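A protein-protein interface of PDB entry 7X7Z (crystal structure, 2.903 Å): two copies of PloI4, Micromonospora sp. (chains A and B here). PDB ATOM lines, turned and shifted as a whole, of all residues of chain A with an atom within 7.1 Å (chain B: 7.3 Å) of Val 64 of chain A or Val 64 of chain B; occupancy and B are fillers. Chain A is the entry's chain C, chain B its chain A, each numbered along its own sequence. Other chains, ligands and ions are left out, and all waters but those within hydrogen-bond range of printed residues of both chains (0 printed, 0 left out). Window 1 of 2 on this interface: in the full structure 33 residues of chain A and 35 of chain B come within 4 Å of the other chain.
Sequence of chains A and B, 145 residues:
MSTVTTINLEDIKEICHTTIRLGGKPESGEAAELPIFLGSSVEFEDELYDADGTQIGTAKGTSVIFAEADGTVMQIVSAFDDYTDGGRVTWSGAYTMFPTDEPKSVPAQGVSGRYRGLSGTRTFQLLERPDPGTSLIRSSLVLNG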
ATOM      1  N   PHE A  37       2.577  35.131   3.497  1.00  0.00           N
ATOM      2  CA  PHE A  37       2.508  35.898   2.262  1.00  0.00           C
ATOM      3  C   PHE A  37       2.140  34.978   1.109  1.00  0.00           C
ATOM      4  O   PHE A  37       2.757  33.924   0.929  1.00  0.00           O
ATOM      5  CB  PHE A  37       3.837  36.604   1.971  1.00  0.00           C
ATOM      6  CG  PHE A  37       4.039  37.862   2.762  1.00  0.00           C
ATOM      7  CD1 PHE A  37       3.473  39.057   2.346  1.00  0.00           C
ATOM      8  CD2 PHE A  37       4.791  37.850   3.923  1.00  0.00           C
ATOM      9  CE1 PHE A  37       3.656  40.216   3.075  1.00  0.00           C
ATOM     10  CE2 PHE A  37       4.979  39.006   4.657  1.00  0.00           C
ATOM     11  CZ  PHE A  37       4.410  40.190   4.231  1.00  0.00           C
ATOM     12  N   LEU A  38       1.132  35.379   0.338  1.00  0.00           N
ATOM     13  CA  LEU A  38       0.790  34.690  -0.898  1.00  0.00           C
ATOM     14  C   LEU A  38       1.797  35.073  -1.974  1.00  0.00           C
ATOM     15  O   LEU A  38       1.953  36.257  -2.290  1.00  0.00           O
ATOM     16  CB  LEU A  38      -0.624  35.050  -1.343  1.00  0.00           C
ATOM     17  CG  LEU A  38      -1.732  34.842  -0.314  1.00  0.00           C
ATOM     18  CD1 LEU A  38      -2.960  35.665  -0.682  1.00  0.00           C
ATOM     19  CD2 LEU A  38      -2.063  33.367  -0.214  1.00  0.00           C
ATOM     20  N   GLY A  39       2.481  34.079  -2.533  1.00  0.00           N
ATOM     21  CA  GLY A  39       3.451  34.356  -3.570  1.00  0.00           C
ATOM     22  C   GLY A  39       2.803  34.741  -4.885  1.00  0.00           C
ATOM     23  O   GLY A  39       1.659  34.394  -5.183  1.00  0.00           O
ATOM     24  N   SER A  40       3.560  35.486  -5.688  1.00  0.00           N
ATOM     25  CA  SER A  40       3.108  35.827  -7.029  1.00  0.00           C
ATOM     26  C   SER A  40       3.027  34.559  -7.869  1.00  0.00           C
ATOM     27  O   SER A  40       4.034  33.873  -8.070  1.00  0.00           O
ATOM     28  CB  SER A  40       4.048  36.848  -7.665  1.00  0.00           C
ATOM     29  OG  SER A  40       4.183  37.997  -6.847  1.00  0.00           O
ATOM     30  N   SER A  41       1.830  34.248  -8.349  1.00  0.00           N
ATOM     31  CA  SER A  41       1.563  32.994  -9.035  1.00  0.00           C
ATOM     32  C   SER A  41       1.472  33.203 -10.541  1.00  0.00           C
ATOM     33  O   SER A  41       1.150  34.292 -11.022  1.00  0.00           O
ATOM     34  CB  SER A  41       0.264  32.368  -8.521  1.00  0.00           C
ATOM     35  OG  SER A  41      -0.838  32.752  -9.326  1.00  0.00           O
ATOM     36  N   VAL A  42       1.780  32.141 -11.284  1.00  0.00           N
ATOM     37  CA  VAL A  42       1.570  32.089 -12.727  1.00  0.00           C
ATOM     38  C   VAL A  42       0.990  30.718 -13.050  1.00  0.00           C
ATOM     39  O   VAL A  42       1.678  29.702 -12.907  1.00  0.00           O
ATOM     40  CB  VAL A  42       2.857  32.326 -13.535  1.00  0.00           C
ATOM     41  CG1 VAL A  42       2.545  32.303 -15.028  1.00  0.00           C
ATOM     42  CG2 VAL A  42       3.508  33.647 -13.153  1.00  0.00           C
ATOM     43  N   THR A  62       1.810  25.453 -12.943  1.00  0.00           N
ATOM     44  CA  THR A  62       1.718  26.578 -12.024  1.00  0.00           C
ATOM     45  C   THR A  62       3.119  26.952 -11.561  1.00  0.00           C
ATOM     46  O   THR A  62       3.963  26.076 -11.348  1.00  0.00           O
ATOM     47  CB  THR A  62       0.826  26.231 -10.816  1.00  0.00           C
ATOM     48  OG1 THR A  62      -0.502  25.934 -11.267  1.00  0.00           O
ATOM     49  CG2 THR A  62       0.766  27.386  -9.826  1.00  0.00           C
ATOM     50  N   SER A  63       3.369  28.254 -11.419  1.00  0.00           N
ATOM     51  CA  SER A  63       4.664  28.753 -10.972  1.00  0.00           C
ATOM     52  C   SER A  63       4.458  29.828  -9.914  1.00  0.00           C
ATOM     53  O   SER A  63       3.630  30.726 -10.095  1.00  0.00           O
ATOM     54  CB  SER A  63       5.475  29.307 -12.145  1.00  0.00           C
ATOM     55  OG  SER A  63       6.693  29.868 -11.695  1.00  0.00           O
ATOM     56  N   VAL A  64       5.206  29.731  -8.813  1.00  0.00           N
ATOM     57  CA  VAL A  64       5.091  30.656  -7.691  1.00  0.00           C
ATOM     58  C   VAL A  64       6.478  31.172  -7.325  1.00  0.00           C
ATOM     59  O   VAL A  64       7.480  30.465  -7.462  1.00  0.00           O
ATOM     60  CB  VAL A  64       4.415  29.994  -6.467  1.00  0.00           C
ATOM     61  CG1 VAL A  64       4.137  31.023  -5.380  1.00  0.00           C
ATOM     62  CG2 VAL A  64       3.127  29.301  -6.877  1.00  0.00           C
ATOM     63  N   ILE A  65       6.527  32.418  -6.852  1.00  0.00           N
ATOM     64  CA  ILE A  65       7.774  33.070  -6.468  1.00  0.00           C
ATOM     65  C   ILE A  65       8.014  32.874  -4.978  1.00  0.00           C
ATOM     66  O   ILE A  65       7.087  32.969  -4.165  1.00  0.00           O
ATOM     67  CB  ILE A  65       7.739  34.567  -6.825  1.00  0.00           C
ATOM     68  CG1 ILE A  65       7.440  34.759  -8.312  1.00  0.00           C
ATOM     69  CG2 ILE A  65       9.053  35.240  -6.448  1.00  0.00           C
ATOM     70  CD1 ILE A  65       7.519  36.200  -8.767  1.00  0.00           C
ATOM     71  N   PHE A  66       9.264  32.598  -4.618  1.00  0.00           N
ATOM     72  CA  PHE A  66       9.692  32.559  -3.225  1.00  0.00           C
ATOM     73  C   PHE A  66      11.158  32.974  -3.176  1.00  0.00           C
ATOM     74  O   PHE A  66      11.715  33.461  -4.164  1.00  0.00           O
ATOM     75  CB  PHE A  66       9.436  31.177  -2.608  1.00  0.00           C
ATOM     76  CG  PHE A  66      10.361  30.100  -3.104  1.00  0.00           C
ATOM     77  CD1 PHE A  66      10.200  29.554  -4.367  1.00  0.00           C
ATOM     78  CD2 PHE A  66      11.381  29.620  -2.297  1.00  0.00           C
ATOM     79  CE1 PHE A  66      11.044  28.558  -4.821  1.00  0.00           C
ATOM     80  CE2 PHE A  66      12.229  28.625  -2.745  1.00  0.00           C
ATOM     81  CZ  PHE A  66      12.060  28.093  -4.008  1.00  0.00           C
ATOM     82  N   ALA A  67      11.788  32.791  -2.018  1.00  0.00           N
ATOM     83  CA  ALA A  67      13.162  33.229  -1.823  1.00  0.00           C
ATOM     84  C   ALA A  67      13.923  32.204  -0.997  1.00  0.00           C
ATOM     85  O   ALA A  67      13.336  31.443  -0.222  1.00  0.00           O
ATOM     86  CB  ALA A  67      13.224  34.600  -1.137  1.00  0.00           C
ATOM     87  N   MET A  74      13.568  33.182  -5.959  1.00  0.00           N
ATOM     88  CA  MET A  74      13.433  31.902  -6.635  1.00  0.00           C
ATOM     89  C   MET A  74      12.053  31.763  -7.266  1.00  0.00           C
ATOM     90  O   MET A  74      11.175  32.616  -7.115  1.00  0.00           O
ATOM     91  CB  MET A  74      13.682  30.746  -5.660  1.00  0.00           C
ATOM     92  CG  MET A  74      15.073  30.723  -5.070  1.00  0.00           C
ATOM     93  SD  MET A  74      16.337  30.339  -6.294  1.00  0.00           S
ATOM     94  CE  MET A  74      16.066  28.583  -6.522  1.00  0.00           C
ATOM     95  N   GLN A  75      11.878  30.652  -7.977  1.00  0.00           N
ATOM     96  CA  GLN A  75      10.619  30.339  -8.641  1.00  0.00           C
ATOM     97  C   GLN A  75      10.450  28.829  -8.636  1.00  0.00           C
ATOM     98  O   GLN A  75      11.318  28.110  -9.139  1.00  0.00           O
ATOM     99  CB  GLN A  75      10.608  30.881 -10.072  1.00  0.00           C
ATOM    100  CG  GLN A  75       9.255  31.369 -10.550  1.00  0.00           C
ATOM    101  CD  GLN A  75       9.363  32.281 -11.755  1.00  0.00           C
ATOM    102  OE1 GLN A  75       8.922  31.937 -12.851  1.00  0.00           O
ATOM    103  NE2 GLN A  75       9.952  33.454 -11.558  1.00  0.00           N
ATOM    104  N   ILE A  76       9.352  28.349  -8.062  1.00  0.00           N
ATOM    105  CA  ILE A  76       9.035  26.925  -8.046  1.00  0.00           C
ATOM    106  C   ILE A  76       7.963  26.658  -9.091  1.00  0.00           C
ATOM    107  O   ILE A  76       7.019  27.444  -9.244  1.00  0.00           O
ATOM    108  CB  ILE A  76       8.587  26.464  -6.643  1.00  0.00           C
ATOM    109  CG1 ILE A  76       8.374  24.948  -6.620  1.00  0.00           C
ATOM    110  CG2 ILE A  76       7.329  27.202  -6.200  1.00  0.00           C
ATOM    111  CD1 ILE A  76       8.215  24.375  -5.229  1.00  0.00           C
ATOM    112  N   VAL A  77       8.114  25.562  -9.830  1.00  0.00           N
ATOM    113  CA  VAL A  77       7.201  25.219 -10.912  1.00  0.00           C
ATOM    114  C   VAL A  77       6.771  23.766 -10.766  1.00  0.00           C
ATOM    115  O   VAL A  77       7.572  22.900 -10.400  1.00  0.00           O
ATOM    116  CB  VAL A  77       7.839  25.470 -12.298  1.00  0.00           C
ATOM    117  CG1 VAL A  77       9.053  24.573 -12.514  1.00  0.00           C
ATOM    118  CG2 VAL A  77       6.814  25.272 -13.403  1.00  0.00           C
ATOM    119  N   SER A  78       5.490  23.512 -11.025  1.00  0.00           N
ATOM    120  CA  SER A  78       4.955  22.164 -11.157  1.00  0.00           C
ATOM    121  C   SER A  78       4.148  22.122 -12.442  1.00  0.00           C
ATOM    122  O   SER A  78       3.183  22.877 -12.592  1.00  0.00           O
ATOM    123  CB  SER A  78       4.086  21.779  -9.960  1.00  0.00           C
ATOM    124  OG  SER A  78       3.648  20.436 -10.075  1.00  0.00           O
ATOM    125  N   TYR A  95      14.079  27.208  -9.555  1.00  0.00           N
ATOM    126  CA  TYR A  95      15.131  27.893 -10.287  1.00  0.00           C
ATOM    127  C   TYR A  95      15.154  29.353  -9.860  1.00  0.00           C
ATOM    128  O   TYR A  95      14.173  29.877  -9.326  1.00  0.00           O
ATOM    129  CB  TYR A  95      14.930  27.783 -11.807  1.00  0.00           C
ATOM    130  CG  TYR A  95      13.538  28.158 -12.269  1.00  0.00           C
ATOM    131  CD1 TYR A  95      13.254  29.446 -12.703  1.00  0.00           C
ATOM    132  CD2 TYR A  95      12.507  27.225 -12.270  1.00  0.00           C
ATOM    133  CE1 TYR A  95      11.984  29.796 -13.123  1.00  0.00           C
ATOM    134  CE2 TYR A  95      11.233  27.566 -12.687  1.00  0.00           C
ATOM    135  CZ  TYR A  95      10.977  28.853 -13.112  1.00  0.00           C
ATOM    136  OH  TYR A  95       9.711  29.198 -13.529  1.00  0.00           O
ATOM    137  N   PHE B  37       5.690  39.367  -5.024  1.00  0.00           N
ATOM    138  CA  PHE B  37       5.682  38.990  -3.618  1.00  0.00           C
ATOM    139  C   PHE B  37       6.321  37.619  -3.471  1.00  0.00           C
ATOM    140  O   PHE B  37       5.966  36.685  -4.198  1.00  0.00           O
ATOM    141  CB  PHE B  37       4.257  38.962  -3.051  1.00  0.00           C
ATOM    142  CG  PHE B  37       3.757  40.301  -2.596  1.00  0.00           C
ATOM    143  CD1 PHE B  37       4.142  40.818  -1.371  1.00  0.00           C
ATOM    144  CD2 PHE B  37       2.891  41.039  -3.386  1.00  0.00           C
ATOM    145  CE1 PHE B  37       3.680  42.047  -0.946  1.00  0.00           C
ATOM    146  CE2 PHE B  37       2.426  42.270  -2.966  1.00  0.00           C
ATOM    147  CZ  PHE B  37       2.821  42.774  -1.744  1.00  0.00           C
ATOM    148  N   LEU B  38       7.262  37.501  -2.540  1.00  0.00           N
ATOM    149  CA  LEU B  38       7.843  36.206  -2.208  1.00  0.00           C
ATOM    150  C   LEU B  38       6.889  35.476  -1.273  1.00  0.00           C
ATOM    151  O   LEU B  38       6.647  35.922  -0.145  1.00  0.00           O
ATOM    152  CB  LEU B  38       9.217  36.369  -1.567  1.00  0.00           C
ATOM    153  CG  LEU B  38      10.159  37.428  -2.136  1.00  0.00           C
ATOM    154  CD1 LEU B  38      11.223  37.813  -1.114  1.00  0.00           C
ATOM    155  CD2 LEU B  38      10.802  36.932  -3.417  1.00  0.00           C
ATOM    156  N   GLY B  39       6.341  34.357  -1.739  1.00  0.00           N
ATOM    157  CA  GLY B  39       5.478  33.562  -0.887  1.00  0.00           C
ATOM    158  C   GLY B  39       6.238  32.931   0.261  1.00  0.00           C
ATOM    159  O   GLY B  39       7.445  32.686   0.183  1.00  0.00           O
ATOM    160  N   SER B  40       5.517  32.666   1.347  1.00  0.00           N
ATOM    161  CA  SER B  40       6.112  31.972   2.477  1.00  0.00           C
ATOM    162  C   SER B  40       6.453  30.542   2.079  1.00  0.00           C
ATOM    163  O   SER B  40       5.608  29.822   1.539  1.00  0.00           O
ATOM    164  CB  SER B  40       5.160  31.991   3.674  1.00  0.00           C
ATOM    165  OG  SER B  40       4.835  33.320   4.048  1.00  0.00           O
ATOM    166  N   SER B  41       7.689  30.132   2.344  1.00  0.00           N
ATOM    167  CA  SER B  41       8.204  28.867   1.850  1.00  0.00           C
ATOM    168  C   SER B  41       8.566  27.933   2.998  1.00  0.00           C
ATOM    169  O   SER B  41       8.849  28.370   4.119  1.00  0.00           O
ATOM    170  CB  SER B  41       9.436  29.085   0.960  1.00  0.00           C
ATOM    171  OG  SER B  41      10.307  30.049   1.518  1.00  0.00           O
ATOM    172  N   VAL B  42       8.548  26.632   2.705  1.00  0.00           N
ATOM    173  CA  VAL B  42       8.983  25.596   3.637  1.00  0.00           C
ATOM    174  C   VAL B  42       9.889  24.634   2.883  1.00  0.00           C
ATOM    175  O   VAL B  42       9.449  23.978   1.931  1.00  0.00           O
ATOM    176  CB  VAL B  42       7.802  24.834   4.265  1.00  0.00           C
ATOM    177  CG1 VAL B  42       8.290  23.978   5.428  1.00  0.00           C
ATOM    178  CG2 VAL B  42       6.715  25.793   4.733  1.00  0.00           C
ATOM    179  N   THR B  62      10.377  21.325  -1.371  1.00  0.00           N
ATOM    180  CA  THR B  62      10.068  22.714  -1.061  1.00  0.00           C
ATOM    181  C   THR B  62       8.588  22.964  -1.305  1.00  0.00           C
ATOM    182  O   THR B  62       8.020  22.466  -2.282  1.00  0.00           O
ATOM    183  CB  THR B  62      10.910  23.673  -1.917  1.00  0.00           C
ATOM    184  OG1 THR B  62      12.301  23.470  -1.641  1.00  0.00           O
ATOM    185  CG2 THR B  62      10.550  25.122  -1.627  1.00  0.00           C
ATOM    186  N   SER B  63       7.963  23.733  -0.413  1.00  0.00           N
ATOM    187  CA  SER B  63       6.563  24.110  -0.543  1.00  0.00           C
ATOM    188  C   SER B  63       6.427  25.618  -0.391  1.00  0.00           C
ATOM    189  O   SER B  63       7.065  26.220   0.478  1.00  0.00           O
ATOM    190  CB  SER B  63       5.695  23.396   0.495  1.00  0.00           C
ATOM    191  OG  SER B  63       4.366  23.250   0.027  1.00  0.00           O
ATOM    192  N   VAL B  64       5.601  26.227  -1.242  1.00  0.00           N
ATOM    193  CA  VAL B  64       5.392  27.670  -1.248  1.00  0.00           C
ATOM    194  C   VAL B  64       3.897  27.958  -1.222  1.00  0.00           C
ATOM    195  O   VAL B  64       3.091  27.211  -1.784  1.00  0.00           O
ATOM    196  CB  VAL B  64       6.056  28.342  -2.475  1.00  0.00           C
ATOM    197  CG1 VAL B  64       6.003  29.859  -2.353  1.00  0.00           C
ATOM    198  CG2 VAL B  64       7.494  27.876  -2.627  1.00  0.00           C
ATOM    199  N   ILE B  65       3.529  29.060  -0.564  1.00  0.00           N
ATOM    200  CA  ILE B  65       2.135  29.457  -0.397  1.00  0.00           C
ATOM    201  C   ILE B  65       1.738  30.423  -1.504  1.00  0.00           C
ATOM    202  O   ILE B  65       2.495  31.335  -1.860  1.00  0.00           O
ATOM    203  CB  ILE B  65       1.916  30.086   0.991  1.00  0.00           C
ATOM    204  CG1 ILE B  65       2.258  29.084   2.093  1.00  0.00           C
ATOM    205  CG2 ILE B  65       0.482  30.576   1.140  1.00  0.00           C
ATOM    206  CD1 ILE B  65       1.983  29.595   3.488  1.00  0.00           C
ATOM    207  N   PHE B  66       0.540  30.223  -2.052  1.00  0.00           N
ATOM    208  CA  PHE B  66      -0.039  31.133  -3.031  1.00  0.00           C
ATOM    209  C   PHE B  66      -1.557  31.019  -2.953  1.00  0.00           C
ATOM    210  O   PHE B  66      -2.101  30.207  -2.199  1.00  0.00           O
ATOM    211  CB  PHE B  66       0.482  30.841  -4.443  1.00  0.00           C
ATOM    212  CG  PHE B  66      -0.081  29.591  -5.058  1.00  0.00           C
ATOM    213  CD1 PHE B  66       0.275  28.342  -4.577  1.00  0.00           C
ATOM    214  CD2 PHE B  66      -0.961  29.663  -6.127  1.00  0.00           C
ATOM    215  CE1 PHE B  66      -0.237  27.191  -5.144  1.00  0.00           C
ATOM    216  CE2 PHE B  66      -1.477  28.515  -6.698  1.00  0.00           C
ATOM    217  CZ  PHE B  66      -1.113  27.278  -6.205  1.00  0.00           C
ATOM    218  N   ALA B  67      -2.243  31.848  -3.734  1.00  0.00           N
ATOM    219  CA  ALA B  67      -3.697  31.891  -3.740  1.00  0.00           C
ATOM    220  C   ALA B  67      -4.229  31.671  -5.149  1.00  0.00           C
ATOM    221  O   ALA B  67      -3.520  31.854  -6.143  1.00  0.00           O
ATOM    222  CB  ALA B  67      -4.218  33.225  -3.190  1.00  0.00           C
ATOM    223  N   MET B  74      -3.391  28.342  -1.180  1.00  0.00           N
ATOM    224  CA  MET B  74      -2.925  27.052  -1.663  1.00  0.00           C
ATOM    225  C   MET B  74      -1.429  26.909  -1.413  1.00  0.00           C
ATOM    226  O   MET B  74      -0.730  27.875  -1.095  1.00  0.00           O
ATOM    227  CB  MET B  74      -3.209  26.876  -3.161  1.00  0.00           C
ATOM    228  CG  MET B  74      -4.661  27.094  -3.546  1.00  0.00           C
ATOM    229  SD  MET B  74      -5.482  25.547  -3.958  1.00  0.00           S
ATOM    230  CE  MET B  74      -4.673  25.158  -5.507  1.00  0.00           C
ATOM    231  N   GLN B  75      -0.945  25.681  -1.571  1.00  0.00           N
ATOM    232  CA  GLN B  75       0.477  25.383  -1.520  1.00  0.00           C
ATOM    233  C   GLN B  75       0.859  24.558  -2.737  1.00  0.00           C
ATOM    234  O   GLN B  75       0.157  23.609  -3.101  1.00  0.00           O
ATOM    235  CB  GLN B  75       0.859  24.623  -0.245  1.00  0.00           C
ATOM    236  CG  GLN B  75       0.502  25.326   1.051  1.00  0.00           C
ATOM    237  CD  GLN B  75       1.238  24.740   2.239  1.00  0.00           C
ATOM    238  OE1 GLN B  75       0.633  24.135   3.124  1.00  0.00           O
ATOM    239  NE2 GLN B  75       2.555  24.913   2.262  1.00  0.00           N
ATOM    240  N   ILE B  76       1.967  24.930  -3.366  1.00  0.00           N
ATOM    241  CA  ILE B  76       2.592  24.125  -4.406  1.00  0.00           C
ATOM    242  C   ILE B  76       3.844  23.499  -3.811  1.00  0.00           C
ATOM    243  O   ILE B  76       4.602  24.164  -3.095  1.00  0.00           O
ATOM    244  CB  ILE B  76       2.920  24.960  -5.663  1.00  0.00           C
ATOM    245  CG1 ILE B  76       3.536  24.075  -6.749  1.00  0.00           C
ATOM    246  CG2 ILE B  76       3.839  26.125  -5.322  1.00  0.00           C
ATOM    247  CD1 ILE B  76       3.908  24.825  -8.006  1.00  0.00           C
ATOM    248  N   VAL B  77       4.043  22.214  -4.077  1.00  0.00           N
ATOM    249  CA  VAL B  77       5.178  21.479  -3.537  1.00  0.00           C
ATOM    250  C   VAL B  77       5.915  20.803  -4.683  1.00  0.00           C
ATOM    251  O   VAL B  77       5.294  20.302  -5.626  1.00  0.00           O
ATOM    252  CB  VAL B  77       4.741  20.448  -2.472  1.00  0.00           C
ATOM    253  CG1 VAL B  77       3.787  19.418  -3.065  1.00  0.00           C
ATOM    254  CG2 VAL B  77       5.954  19.770  -1.852  1.00  0.00           C
ATOM    255  N   SER B  78       7.244  20.825  -4.615  1.00  0.00           N
ATOM    256  CA  SER B  78       8.100  20.048  -5.502  1.00  0.00           C
ATOM    257  C   SER B  78       9.055  19.252  -4.629  1.00  0.00           C
ATOM    258  O   SER B  78       9.833  19.836  -3.869  1.00  0.00           O
ATOM    259  CB  SER B  78       8.868  20.945  -6.472  1.00  0.00           C
ATOM    260  OG  SER B  78       9.853  20.202  -7.168  1.00  0.00           O
ATOM    261  N   TYR B  95      -2.103  21.945  -3.798  1.00  0.00           N
ATOM    262  CA  TYR B  95      -3.166  21.526  -2.899  1.00  0.00           C
ATOM    263  C   TYR B  95      -3.583  22.724  -2.061  1.00  0.00           C
ATOM    264  O   TYR B  95      -2.832  23.693  -1.913  1.00  0.00           O
ATOM    265  CB  TYR B  95      -2.725  20.361  -2.003  1.00  0.00           C
ATOM    266  CG  TYR B  95      -1.487  20.655  -1.184  1.00  0.00           C
ATOM    267  CD1 TYR B  95      -1.587  21.138   0.114  1.00  0.00           C
ATOM    268  CD2 TYR B  95      -0.218  20.453  -1.711  1.00  0.00           C
ATOM    269  CE1 TYR B  95      -0.459  21.411   0.864  1.00  0.00           C
ATOM    270  CE2 TYR B  95       0.916  20.724  -0.969  1.00  0.00           C
ATOM    271  CZ  TYR B  95       0.790  21.201   0.318  1.00  0.00           C
ATOM    272  OH  TYR B  95       1.916  21.473   1.061  1.00  0.00           O
ATOM    273  N   MET B  97      -4.215  24.774   1.242  1.00  0.00           N
ATOM    274  CA  MET B  97      -3.503  24.780   2.514  1.00  0.00           C
ATOM    275  C   MET B  97      -4.425  24.421   3.673  1.00  0.00           C
ATOM    276  O   MET B  97      -4.026  23.685   4.586  1.00  0.00           O
ATOM    277  CB  MET B  97      -2.857  26.145   2.745  1.00  0.00           C
ATOM    278  CG  MET B  97      -2.371  26.360   4.165  1.00  0.00           C
ATOM    279  SD  MET B  97      -0.883  27.368   4.244  1.00  0.00           S
ATOM    280  CE  MET B  97      -1.594  28.987   4.486  1.00  0.00           C
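C of Leu 38 of chain A touches O of Ile 65 of chain B (3.8 Å). Gly 39 of chain B touches Gly 39 of chain A. Phe 66 of chain B touches Ser 41 of chain A (CD2 to CB, 3.8 Å). CG1 of Val 64 of chain B touches CG1 of Val 64 of chain A, at 3.7 Å. O of Ile 65 of chain B touches CG1 of Val 64 of chain A, 3.9 Å away. Val 64 of chain A touches Phe 66 of chain B. Ile 65 of chain A touches Phe 37 of chain B (CB to O, 3.8 Å). CD2 of Leu 38 of chain B touches O of Phe 66 of chain A (3.7 Å). Phe 66 of chain A touches Ser 41 of chain B. Ala 67 of chain A touches Ser 41 of chain B.
The side-chain hydroxyl of Ser 63 of chain A lies close to the backbone carbonyl oxygen of Ile 76 of chain A (3.5 Å). The backbone carbonyl oxygen of Val 64 of chain A lies within hydrogen-bond range of the backbone NH of Ile 76 of chain A (2.9 Å). The backbone carbonyl oxygen of Phe 66 of chain A sits at hydrogen-bond distance from the backbone NH of Met 74 of chain A (2.6 Å). The side-chain hydroxyl (OG) of Ser 63 of chain B lies close to the backbone carbonyl oxygen (O) of Ile 76 of chain B (3.3 Å). N of Val 64 of chain B is in hydrogen-bond range of O of Ile 76 of chain B, at 2.9 Å. The backbone carbonyl oxygen of Ser 40 of chain A sits at hydrogen-bond distance from the backbone NH of Ile 65 of chain A, 3.1 Å away.
Phe 37 of chain A touches Ser 40 of chain B, and with the chains exchanged Ser 40 of chain A touches Phe 37 of chain B. Leu 38 of chain A touches Ala 67 of chain B, and with the chains exchanged Ala 67 of chain A touches Leu 38 of chain B. Gly 39 of chain A touches Ile 65 of chain B, and with the chains exchanged Ile 65 of chain A touches Gly 39 of chain B. Val 64 of chain A touches Ile 76 of chain B, and with the chains exchanged Ile 76 of chain A touches Val 64 of chain B.
N of Gly 39 of chain B lies within hydrogen-bond range of O of Ile 65 of chain A (2.9 Å). The backbone NH (N) of Phe 37 of chain B lies within hydrogen-bond range of the side-chain hydroxyl (OG) of Ser 40 of chain A (2.7 Å). OG of Ser 40 of chain B lies within hydrogen-bond range of N of Phe 37 of chain A, at 2.9 Å. The backbone carbonyl oxygen (O) of Ile 65 of chain B is in hydrogen-bond range of the backbone NH (N) of Gly 39 of chain A.
Of the 19 printed residues of chain B, 12 touch a printed residue of chain A. Hydrophobic or aromatic side chains of chain B that line the printed part of chain A: Phe 37, Leu 38, Val 64, Ile 65, Phe 66, Ala 67 and Ile 76. Of the 18 printed residues of chain A, 12 touch a printed residue of chain B. Hydrophobic or aromatic side chains of chain A within 4 Å of the printed part of chain B: Phe 37, Leu 38, Val 64, Ile 65, Phe 66, Ala 67 and Ile 76. Among the printed residues, no Asp or Glu carboxylate lies within 4 Å of a Lys or Arg side-chain nitrogen of the other chain.
Of chain B, only Val 64, Ile 65, Phe 66 and Ile 76 come within 4 Å of Val 64 of chain A. Of the printed residues of chain B, Ile 76 of chain A touches Thr 62 (3.5 Å), Val 64 (3.6 Å), Ile 76 (3.8 Å) and Ser 78 (3.7 Å). Printed residues of chain B within 4 Å of Ser 78 of chain A: Ile 76 (3.6 Å). Printed residues of chain A within 4 Å of Leu 38 of chain B: Phe 37 (3.6 Å), Ile 65 (3.8 Å), Phe 66 (3.7 Å) and Ala 67 (3.8 Å). Printed residues of chain A within 4 Å of Thr 62 of chain B: Ile 76 (3.5 Å). Of the printed residues of chain A, Val 64 of chain B touches Val 64, Ile 65, Phe 66 and Ile 76. Gln 75 of chain B touches none of the printed residues of chain A. Tyr 95 of chain B touches none of the printed residues of chain A. The nearest residue of chain B that does not touch Val 64 of chain A is Gly 39 of chain B (5.3 Å). The nearest printed residue of chain B that does not touch Phe 37 of chain A is Phe 37 of chain B (4.2 Å).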
